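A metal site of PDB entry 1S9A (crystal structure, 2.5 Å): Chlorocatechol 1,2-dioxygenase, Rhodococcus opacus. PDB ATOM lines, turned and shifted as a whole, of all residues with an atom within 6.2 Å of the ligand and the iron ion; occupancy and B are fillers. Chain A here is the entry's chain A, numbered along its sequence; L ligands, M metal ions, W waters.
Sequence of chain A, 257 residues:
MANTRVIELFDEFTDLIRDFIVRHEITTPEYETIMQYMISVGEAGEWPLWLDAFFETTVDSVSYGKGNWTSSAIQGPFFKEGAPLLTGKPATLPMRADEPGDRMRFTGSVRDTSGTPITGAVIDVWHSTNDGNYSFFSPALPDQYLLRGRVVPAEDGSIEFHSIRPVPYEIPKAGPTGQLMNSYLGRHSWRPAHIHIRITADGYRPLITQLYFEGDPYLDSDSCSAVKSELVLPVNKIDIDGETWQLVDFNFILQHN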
ATOM      1  N   PRO A  48      12.160 -11.099   1.008  1.00  0.00           N
ATOM      2  CA  PRO A  48      11.718 -12.390   1.557  1.00  0.00           C
ATOM      3  C   PRO A  48      11.642 -13.512   0.531  1.00  0.00           C
ATOM      4  O   PRO A  48      12.289 -14.545   0.719  1.00  0.00           O
ATOM      5  CB  PRO A  48      10.334 -12.084   2.120  1.00  0.00           C
ATOM      6  CG  PRO A  48      10.438 -10.661   2.506  1.00  0.00           C
ATOM      7  CD  PRO A  48      11.253 -10.006   1.421  1.00  0.00           C
ATOM      8  N   LEU A  49      10.890 -13.293  -0.551  1.00  0.00           N
ATOM      9  CA  LEU A  49      10.753 -14.270  -1.626  1.00  0.00           C
ATOM     10  C   LEU A  49      12.112 -14.675  -2.235  1.00  0.00           C
ATOM     11  O   LEU A  49      12.389 -15.862  -2.415  1.00  0.00           O
ATOM     12  CB  LEU A  49       9.818 -13.722  -2.720  1.00  0.00           C
ATOM     13  CG  LEU A  49       9.870 -14.312  -4.125  1.00  0.00           C
ATOM     14  CD1 LEU A  49       9.200 -15.650  -4.127  1.00  0.00           C
ATOM     15  CD2 LEU A  49       9.204 -13.401  -5.125  1.00  0.00           C
ATOM     16  N   TRP A  50      12.942 -13.687  -2.535  1.00  0.00           N
ATOM     17  CA  TRP A  50      14.260 -13.902  -3.121  1.00  0.00           C
ATOM     18  C   TRP A  50      15.103 -14.813  -2.203  1.00  0.00           C
ATOM     19  O   TRP A  50      15.542 -15.891  -2.627  1.00  0.00           O
ATOM     20  CB  TRP A  50      14.970 -12.573  -3.375  1.00  0.00           C
ATOM     21  CG  TRP A  50      16.094 -12.690  -4.354  1.00  0.00           C
ATOM     22  CD1 TRP A  50      16.022 -12.469  -5.696  1.00  0.00           C
ATOM     23  CD2 TRP A  50      17.450 -13.053  -4.082  1.00  0.00           C
ATOM     24  NE1 TRP A  50      17.254 -12.676  -6.284  1.00  0.00           N
ATOM     25  CE2 TRP A  50      18.140 -13.034  -5.310  1.00  0.00           C
ATOM     26  CE3 TRP A  50      18.156 -13.370  -2.910  1.00  0.00           C
ATOM     27  CZ2 TRP A  50      19.513 -13.331  -5.409  1.00  0.00           C
ATOM     28  CZ3 TRP A  50      19.525 -13.646  -3.014  1.00  0.00           C
ATOM     29  CH2 TRP A  50      20.180 -13.631  -4.255  1.00  0.00           C
ATOM     30  N   ASP A  52      14.396 -16.541   0.451  1.00  0.00           N
ATOM     31  CA  ASP A  52      13.766 -17.812   0.733  1.00  0.00           C
ATOM     32  C   ASP A  52      13.919 -18.749  -0.444  1.00  0.00           C
ATOM     33  O   ASP A  52      14.080 -19.964  -0.258  1.00  0.00           O
ATOM     34  CB  ASP A  52      12.280 -17.608   1.045  1.00  0.00           C
ATOM     35  CG  ASP A  52      12.019 -17.083   2.441  1.00  0.00           C
ATOM     36  OD1 ASP A  52      12.965 -17.026   3.272  1.00  0.00           O
ATOM     37  OD2 ASP A  52      10.878 -16.718   2.790  1.00  0.00           O
ATOM     38  N   ALA A  53      13.841 -18.195  -1.655  1.00  0.00           N
ATOM     39  CA  ALA A  53      13.925 -19.014  -2.872  1.00  0.00           C
ATOM     40  C   ALA A  53      15.250 -19.737  -2.905  1.00  0.00           C
ATOM     41  O   ALA A  53      15.305 -20.922  -3.189  1.00  0.00           O
ATOM     42  CB  ALA A  53      13.734 -18.174  -4.136  1.00  0.00           C
ATOM     43  N   PHE A  54      16.322 -19.025  -2.557  1.00  0.00           N
ATOM     44  CA  PHE A  54      17.675 -19.558  -2.706  1.00  0.00           C
ATOM     45  C   PHE A  54      18.315 -20.106  -1.442  1.00  0.00           C
ATOM     46  O   PHE A  54      19.106 -21.044  -1.521  1.00  0.00           O
ATOM     47  CB  PHE A  54      18.594 -18.531  -3.370  1.00  0.00           C
ATOM     48  CG  PHE A  54      18.067 -18.017  -4.682  1.00  0.00           C
ATOM     49  CD1 PHE A  54      17.960 -18.862  -5.775  1.00  0.00           C
ATOM     50  CD2 PHE A  54      17.671 -16.699  -4.817  1.00  0.00           C
ATOM     51  CE1 PHE A  54      17.479 -18.398  -6.999  1.00  0.00           C
ATOM     52  CE2 PHE A  54      17.168 -16.219  -6.033  1.00  0.00           C
ATOM     53  CZ  PHE A  54      17.072 -17.072  -7.130  1.00  0.00           C
ATOM     54  N   GLU A  56      16.727 -20.222   2.258  1.00  0.00           N
ATOM     55  CA  GLU A  56      16.004 -20.812   3.391  1.00  0.00           C
ATOM     56  C   GLU A  56      16.174 -22.330   3.494  1.00  0.00           C
ATOM     57  O   GLU A  56      16.111 -22.884   4.599  1.00  0.00           O
ATOM     58  CB  GLU A  56      14.514 -20.446   3.356  1.00  0.00           C
ATOM     59  CG  GLU A  56      13.834 -20.567   4.717  1.00  0.00           C
ATOM     60  CD  GLU A  56      12.326 -20.465   4.626  1.00  0.00           C
ATOM     61  OE1 GLU A  56      11.798 -20.081   3.565  1.00  0.00           O
ATOM     62  OE2 GLU A  56      11.645 -20.765   5.631  1.00  0.00           O
ATOM     63  N   ILE A  74      11.157 -25.681   4.456  1.00  0.00           N
ATOM     64  CA  ILE A  74      11.133 -24.217   4.543  1.00  0.00           C
ATOM     65  C   ILE A  74       9.705 -23.683   4.735  1.00  0.00           C
ATOM     66  O   ILE A  74       8.720 -24.333   4.369  1.00  0.00           O
ATOM     67  CB  ILE A  74      11.870 -23.562   3.325  1.00  0.00           C
ATOM     68  CG1 ILE A  74      11.129 -23.812   1.980  1.00  0.00           C
ATOM     69  CG2 ILE A  74      13.292 -24.083   3.251  1.00  0.00           C
ATOM     70  CD1 ILE A  74      11.581 -22.907   0.797  1.00  0.00           C
ATOM     71  N   GLN A  75       9.592 -22.526   5.366  1.00  0.00           N
ATOM     72  CA  GLN A  75       8.305 -21.890   5.589  1.00  0.00           C
ATOM     73  C   GLN A  75       7.891 -21.084   4.362  1.00  0.00           C
ATOM     74  O   GLN A  75       6.702 -20.915   4.074  1.00  0.00           O
ATOM     75  CB  GLN A  75       8.404 -20.974   6.805  1.00  0.00           C
ATOM     76  CG  GLN A  75       7.106 -20.246   7.145  1.00  0.00           C
ATOM     77  CD  GLN A  75       7.236 -19.321   8.321  1.00  0.00           C
ATOM     78  OE1 GLN A  75       7.740 -19.717   9.365  1.00  0.00           O
ATOM     79  NE2 GLN A  75       6.773 -18.097   8.173  1.00  0.00           N
ATOM     80  N   GLY A  76       8.884 -20.593   3.628  1.00  0.00           N
ATOM     81  CA  GLY A  76       8.654 -19.611   2.594  1.00  0.00           C
ATOM     82  C   GLY A  76       8.175 -18.294   3.185  1.00  0.00           C
ATOM     83  O   GLY A  76       8.008 -18.178   4.410  1.00  0.00           O
ATOM     84  N   PRO A  77       7.941 -17.318   2.297  1.00  0.00           N
ATOM     85  CA  PRO A  77       7.512 -15.959   2.683  1.00  0.00           C
ATOM     86  C   PRO A  77       6.006 -15.758   2.881  1.00  0.00           C
ATOM     87  O   PRO A  77       5.607 -14.676   3.309  1.00  0.00           O
ATOM     88  CB  PRO A  77       7.958 -15.126   1.478  1.00  0.00           C
ATOM     89  CG  PRO A  77       7.751 -16.058   0.309  1.00  0.00           C
ATOM     90  CD  PRO A  77       8.079 -17.436   0.838  1.00  0.00           C
ATOM     91  N   PHE A  78       5.184 -16.761   2.577  1.00  0.00           N
ATOM     92  CA  PHE A  78       3.749 -16.504   2.459  1.00  0.00           C
ATOM     93  C   PHE A  78       2.885 -16.979   3.625  1.00  0.00           C
ATOM     94  O   PHE A  78       1.682 -17.107   3.486  1.00  0.00           O
ATOM     95  CB  PHE A  78       3.227 -17.024   1.096  1.00  0.00           C
ATOM     96  CG  PHE A  78       3.861 -16.343  -0.077  1.00  0.00           C
ATOM     97  CD1 PHE A  78       4.201 -17.061  -1.216  1.00  0.00           C
ATOM     98  CD2 PHE A  78       4.142 -14.988  -0.039  1.00  0.00           C
ATOM     99  CE1 PHE A  78       4.799 -16.429  -2.297  1.00  0.00           C
ATOM    100  CE2 PHE A  78       4.741 -14.342  -1.121  1.00  0.00           C
ATOM    101  CZ  PHE A  78       5.075 -15.066  -2.239  1.00  0.00           C
ATOM    102  N   TRP A 126      -1.667 -23.458   5.210  1.00  0.00           N
ATOM    103  CA  TRP A 126      -1.834 -22.506   4.125  1.00  0.00           C
ATOM    104  C   TRP A 126      -1.304 -23.100   2.825  1.00  0.00           C
ATOM    105  O   TRP A 126      -0.458 -23.983   2.842  1.00  0.00           O
ATOM    106  CB  TRP A 126      -1.207 -21.149   4.444  1.00  0.00           C
ATOM    107  CG  TRP A 126       0.323 -21.036   4.463  1.00  0.00           C
ATOM    108  CD1 TRP A 126       1.117 -20.356   3.573  1.00  0.00           C
ATOM    109  CD2 TRP A 126       1.212 -21.548   5.469  1.00  0.00           C
ATOM    110  NE1 TRP A 126       2.446 -20.443   3.929  1.00  0.00           N
ATOM    111  CE2 TRP A 126       2.539 -21.165   5.095  1.00  0.00           C
ATOM    112  CE3 TRP A 126       1.040 -22.309   6.643  1.00  0.00           C
ATOM    113  CZ2 TRP A 126       3.663 -21.519   5.857  1.00  0.00           C
ATOM    114  CZ3 TRP A 126       2.177 -22.657   7.401  1.00  0.00           C
ATOM    115  CH2 TRP A 126       3.472 -22.257   7.001  1.00  0.00           C
ATOM    116  N   HIS A 127      -1.902 -22.670   1.719  1.00  0.00           N
ATOM    117  CA  HIS A 127      -1.469 -23.079   0.387  1.00  0.00           C
ATOM    118  C   HIS A 127      -1.984 -22.121  -0.681  1.00  0.00           C
ATOM    119  O   HIS A 127      -2.811 -21.263  -0.406  1.00  0.00           O
ATOM    120  CB  HIS A 127      -1.817 -24.540   0.076  1.00  0.00           C
ATOM    121  CG  HIS A 127      -3.282 -24.816  -0.103  1.00  0.00           C
ATOM    122  ND1 HIS A 127      -4.019 -24.305  -1.146  1.00  0.00           N
ATOM    123  CD2 HIS A 127      -4.117 -25.614   0.597  1.00  0.00           C
ATOM    124  CE1 HIS A 127      -5.258 -24.754  -1.061  1.00  0.00           C
ATOM    125  NE2 HIS A 127      -5.348 -25.556  -0.022  1.00  0.00           N
ATOM    126  N   SER A 128      -1.441 -22.244  -1.890  1.00  0.00           N
ATOM    127  CA  SER A 128      -1.795 -21.367  -3.004  1.00  0.00           C
ATOM    128  C   SER A 128      -3.162 -21.707  -3.589  1.00  0.00           C
ATOM    129  O   SER A 128      -3.613 -22.855  -3.502  1.00  0.00           O
ATOM    130  CB  SER A 128      -0.752 -21.511  -4.114  1.00  0.00           C
ATOM    131  OG  SER A 128      -0.786 -22.832  -4.610  1.00  0.00           O
ATOM    132  N   TYR A 134      -1.211 -16.551  -3.146  1.00  0.00           N
ATOM    133  CA  TYR A 134      -1.465 -16.695  -1.718  1.00  0.00           C
ATOM    134  C   TYR A 134      -2.217 -15.470  -1.219  1.00  0.00           C
ATOM    135  O   TYR A 134      -1.886 -14.315  -1.558  1.00  0.00           O
ATOM    136  CB  TYR A 134      -0.143 -16.861  -0.957  1.00  0.00           C
ATOM    137  CG  TYR A 134       0.498 -18.227  -1.060  1.00  0.00           C
ATOM    138  CD1 TYR A 134       1.462 -18.499  -2.027  1.00  0.00           C
ATOM    139  CD2 TYR A 134       0.165 -19.249  -0.174  1.00  0.00           C
ATOM    140  CE1 TYR A 134       2.068 -19.740  -2.108  1.00  0.00           C
ATOM    141  CE2 TYR A 134       0.771 -20.497  -0.243  1.00  0.00           C
ATOM    142  CZ  TYR A 134       1.714 -20.739  -1.228  1.00  0.00           C
ATOM    143  OH  TYR A 134       2.314 -21.986  -1.313  1.00  0.00           O
ATOM    144  N   TYR A 169       3.006 -24.194  -8.879  1.00  0.00           N
ATOM    145  CA  TYR A 169       2.892 -22.760  -9.157  1.00  0.00           C
ATOM    146  C   TYR A 169       4.224 -22.118  -9.470  1.00  0.00           C
ATOM    147  O   TYR A 169       5.277 -22.694  -9.185  1.00  0.00           O
ATOM    148  CB  TYR A 169       2.179 -21.993  -8.037  1.00  0.00           C
ATOM    149  CG  TYR A 169       2.929 -21.852  -6.723  1.00  0.00           C
ATOM    150  CD1 TYR A 169       4.021 -20.974  -6.591  1.00  0.00           C
ATOM    151  CD2 TYR A 169       2.530 -22.572  -5.609  1.00  0.00           C
ATOM    152  CE1 TYR A 169       4.710 -20.840  -5.397  1.00  0.00           C
ATOM    153  CE2 TYR A 169       3.201 -22.443  -4.402  1.00  0.00           C
ATOM    154  CZ  TYR A 169       4.286 -21.588  -4.298  1.00  0.00           C
ATOM    155  OH  TYR A 169       4.919 -21.490  -3.079  1.00  0.00           O
ATOM    156  N   ILE A 171       6.744 -18.591  -9.277  1.00  0.00           N
ATOM    157  CA  ILE A 171       7.124 -17.288  -8.773  1.00  0.00           C
ATOM    158  C   ILE A 171       6.979 -16.320  -9.944  1.00  0.00           C
ATOM    159  O   ILE A 171       7.475 -16.596 -11.044  1.00  0.00           O
ATOM    160  CB  ILE A 171       8.573 -17.342  -8.232  1.00  0.00           C
ATOM    161  CG1 ILE A 171       8.581 -17.980  -6.839  1.00  0.00           C
ATOM    162  CG2 ILE A 171       9.228 -15.951  -8.196  1.00  0.00           C
ATOM    163  CD1 ILE A 171       9.819 -18.801  -6.538  1.00  0.00           C
ATOM    164  N   ARG A 191       7.505 -24.210  -8.395  1.00  0.00           N
ATOM    165  CA  ARG A 191       7.550 -25.069  -7.223  1.00  0.00           C
ATOM    166  C   ARG A 191       6.544 -26.174  -7.489  1.00  0.00           C
ATOM    167  O   ARG A 191       5.517 -25.922  -8.105  1.00  0.00           O
ATOM    168  CB  ARG A 191       7.129 -24.308  -5.949  1.00  0.00           C
ATOM    169  CG  ARG A 191       8.161 -23.324  -5.338  1.00  0.00           C
ATOM    170  CD  ARG A 191       8.283 -23.392  -3.827  1.00  0.00           C
ATOM    171  NE  ARG A 191       8.808 -24.689  -3.449  1.00  0.00           N
ATOM    172  CZ  ARG A 191       8.440 -25.408  -2.387  1.00  0.00           C
ATOM    173  NH1 ARG A 191       7.530 -24.969  -1.538  1.00  0.00           N
ATOM    174  NH2 ARG A 191       8.998 -26.588  -2.186  1.00  0.00           N
ATOM    175  N   HIS A 194       2.156 -28.005  -3.051  1.00  0.00           N
ATOM    176  CA  HIS A 194       2.418 -28.276  -1.650  1.00  0.00           C
ATOM    177  C   HIS A 194       1.369 -27.637  -0.740  1.00  0.00           C
ATOM    178  O   HIS A 194       0.876 -26.523  -1.010  1.00  0.00           O
ATOM    179  CB  HIS A 194       3.821 -27.799  -1.255  1.00  0.00           C
ATOM    180  CG  HIS A 194       4.085 -26.361  -1.590  1.00  0.00           C
ATOM    181  ND1 HIS A 194       4.646 -25.972  -2.782  1.00  0.00           N
ATOM    182  CD2 HIS A 194       3.852 -25.233  -0.894  1.00  0.00           C
ATOM    183  CE1 HIS A 194       4.751 -24.654  -2.808  1.00  0.00           C
ATOM    184  NE2 HIS A 194       4.272 -24.178  -1.669  1.00  0.00           N
ATOM    185  N   HIS A 196       1.565 -26.160   2.920  1.00  0.00           N
ATOM    186  CA  HIS A 196       2.408 -25.759   4.047  1.00  0.00           C
ATOM    187  C   HIS A 196       1.751 -26.148   5.344  1.00  0.00           C
ATOM    188  O   HIS A 196       0.516 -26.104   5.474  1.00  0.00           O
ATOM    189  CB  HIS A 196       2.603 -24.261   4.104  1.00  0.00           C
ATOM    190  CG  HIS A 196       3.315 -23.679   2.926  1.00  0.00           C
ATOM    191  ND1 HIS A 196       4.686 -23.605   2.859  1.00  0.00           N
ATOM    192  CD2 HIS A 196       2.850 -23.070   1.811  1.00  0.00           C
ATOM    193  CE1 HIS A 196       5.040 -22.988   1.736  1.00  0.00           C
ATOM    194  NE2 HIS A 196       3.940 -22.659   1.082  1.00  0.00           N
ATOM    195  N   GLN A 210       6.131 -29.038   4.826  1.00  0.00           N
ATOM    196  CA  GLN A 210       5.375 -28.975   3.584  1.00  0.00           C
ATOM    197  C   GLN A 210       5.028 -30.398   3.181  1.00  0.00           C
ATOM    198  O   GLN A 210       5.811 -31.328   3.407  1.00  0.00           O
ATOM    199  CB  GLN A 210       6.191 -28.322   2.474  1.00  0.00           C
ATOM    200  CG  GLN A 210       6.548 -26.894   2.722  1.00  0.00           C
ATOM    201  CD  GLN A 210       7.221 -26.238   1.531  1.00  0.00           C
ATOM    202  OE1 GLN A 210       6.799 -26.569   0.320  1.00  0.00           O
ATOM    203  NE2 GLN A 210       8.133 -25.427   1.712  1.00  0.00           N
ATOM    204  N   CYS A 224      12.992 -23.569  -5.742  1.00  0.00           N
ATOM    205  CA  CYS A 224      13.306 -23.115  -4.388  1.00  0.00           C
ATOM    206  C   CYS A 224      14.126 -24.115  -3.589  1.00  0.00           C
ATOM    207  O   CYS A 224      14.565 -23.812  -2.486  1.00  0.00           O
ATOM    208  CB  CYS A 224      12.012 -22.782  -3.660  1.00  0.00           C
ATOM    209  SG  CYS A 224      11.320 -21.215  -4.231  1.00  0.00           S
HETATM  210  C1  LIG L   1       6.867 -21.084  -0.983  1.00  0.00           C
HETATM  211  O1  LIG L   1       5.588 -20.470  -0.915  1.00  0.00           O
HETATM  212  O2  LIG L   1       6.934 -22.359  -0.747  1.00  0.00           O
HETATM  213  C2  LIG L   1       8.092 -20.290  -1.306  1.00  0.00           C
HETATM  214  C3  LIG L   1       9.319 -20.663  -0.754  1.00  0.00           C
HETATM  215  C4  LIG L   1      10.457 -19.916  -1.035  1.00  0.00           C
HETATM  216  C5  LIG L   1      10.379 -18.804  -1.873  1.00  0.00           C
HETATM  217  C6  LIG L   1       9.157 -18.445  -2.433  1.00  0.00           C
HETATM  218  C7  LIG L   1       8.013 -19.191  -2.143  1.00  0.00           C
HETATM  219 FE    FE M   1       4.463 -22.253  -1.027  1.00  0.00          FE
HETATM  220  O   HOH W   1       5.154 -19.481   2.298  1.00  0.00           O
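The indole nitrogen (NE1) of Trp 126 lies close to the backbone carbonyl oxygen (O) of Phe 78.
The backbone carbonyl oxygen of Tyr 169 is in hydrogen-bond range of the backbone NH of Arg 191.
OE1 of Gln 210 is in hydrogen-bond range of NH1 of Arg 191 (2.6 Å).
The side-chain amide nitrogen (NE2) of Gln 210 sits at hydrogen-bond distance from the backbone carbonyl oxygen (O) of Ile 74 (2.9 Å).
ND1 of His 194 sits close to NH1 of Arg 191, at 3.3 Å.
The backbone carbonyl oxygen (O) of Trp 126 lies within hydrogen-bond range of the backbone NH (N) of His 196 (3.0 Å).
The side-chain carboxylate (OE1) of Glu 56 sits at hydrogen-bond distance from the backbone NH (N) of Gly 76, 3.0 Å away.
The guanidinium group of Arg 191 lies close to an oxygen (O2) of the ligand (2.8 Å).
The iron ion is bound by a ring nitrogen (NE2) of His 194 (2.0 Å), an oxygen (O1) of the ligand (2.1 Å), the side-chain hydroxyl of Tyr 134 (2.2 Å), a ring nitrogen (NE2) of His 196 (2.2 Å), the side-chain hydroxyl of Tyr 169 (2.2 Å) and an oxygen (O2) of the ligand (2.5 Å).
Leu 49 touches the ligand (CD1 to C6, 3.3 Å).
Asp 52 touches the ligand.
Ala 53 touches the ligand (N to C5, 3.5 Å).
Ile 74 touches the ligand.
Gly 76 touches the ligand.
CD of Pro 77 touches C7 of the ligand, at 3.5 Å.
Phe 78 touches the ligand.
Cys 224 touches the ligand (SG to C5, 3.5 Å).
Hydrophobic or aromatic side chains that line the ligand: Leu 49, Ile 74, Pro 77, Phe 78, Tyr 134, Tyr 169, His 194 and His 196.
The nearest printed residue that does not touch the ligand is Gln 210 (4.1 Å).
Water W1 lies within hydrogen-bond range of the backbone NH (N) of Phe 78, the backbone carbonyl oxygen (O) of Gln 75 and the indole nitrogen (NE1) of Trp 126.
Of the 23 residues printed, 4 come within 4 Å of the iron ion.
Along chain A the residues within 4 Å of the iron ion span positions 134 to 196.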
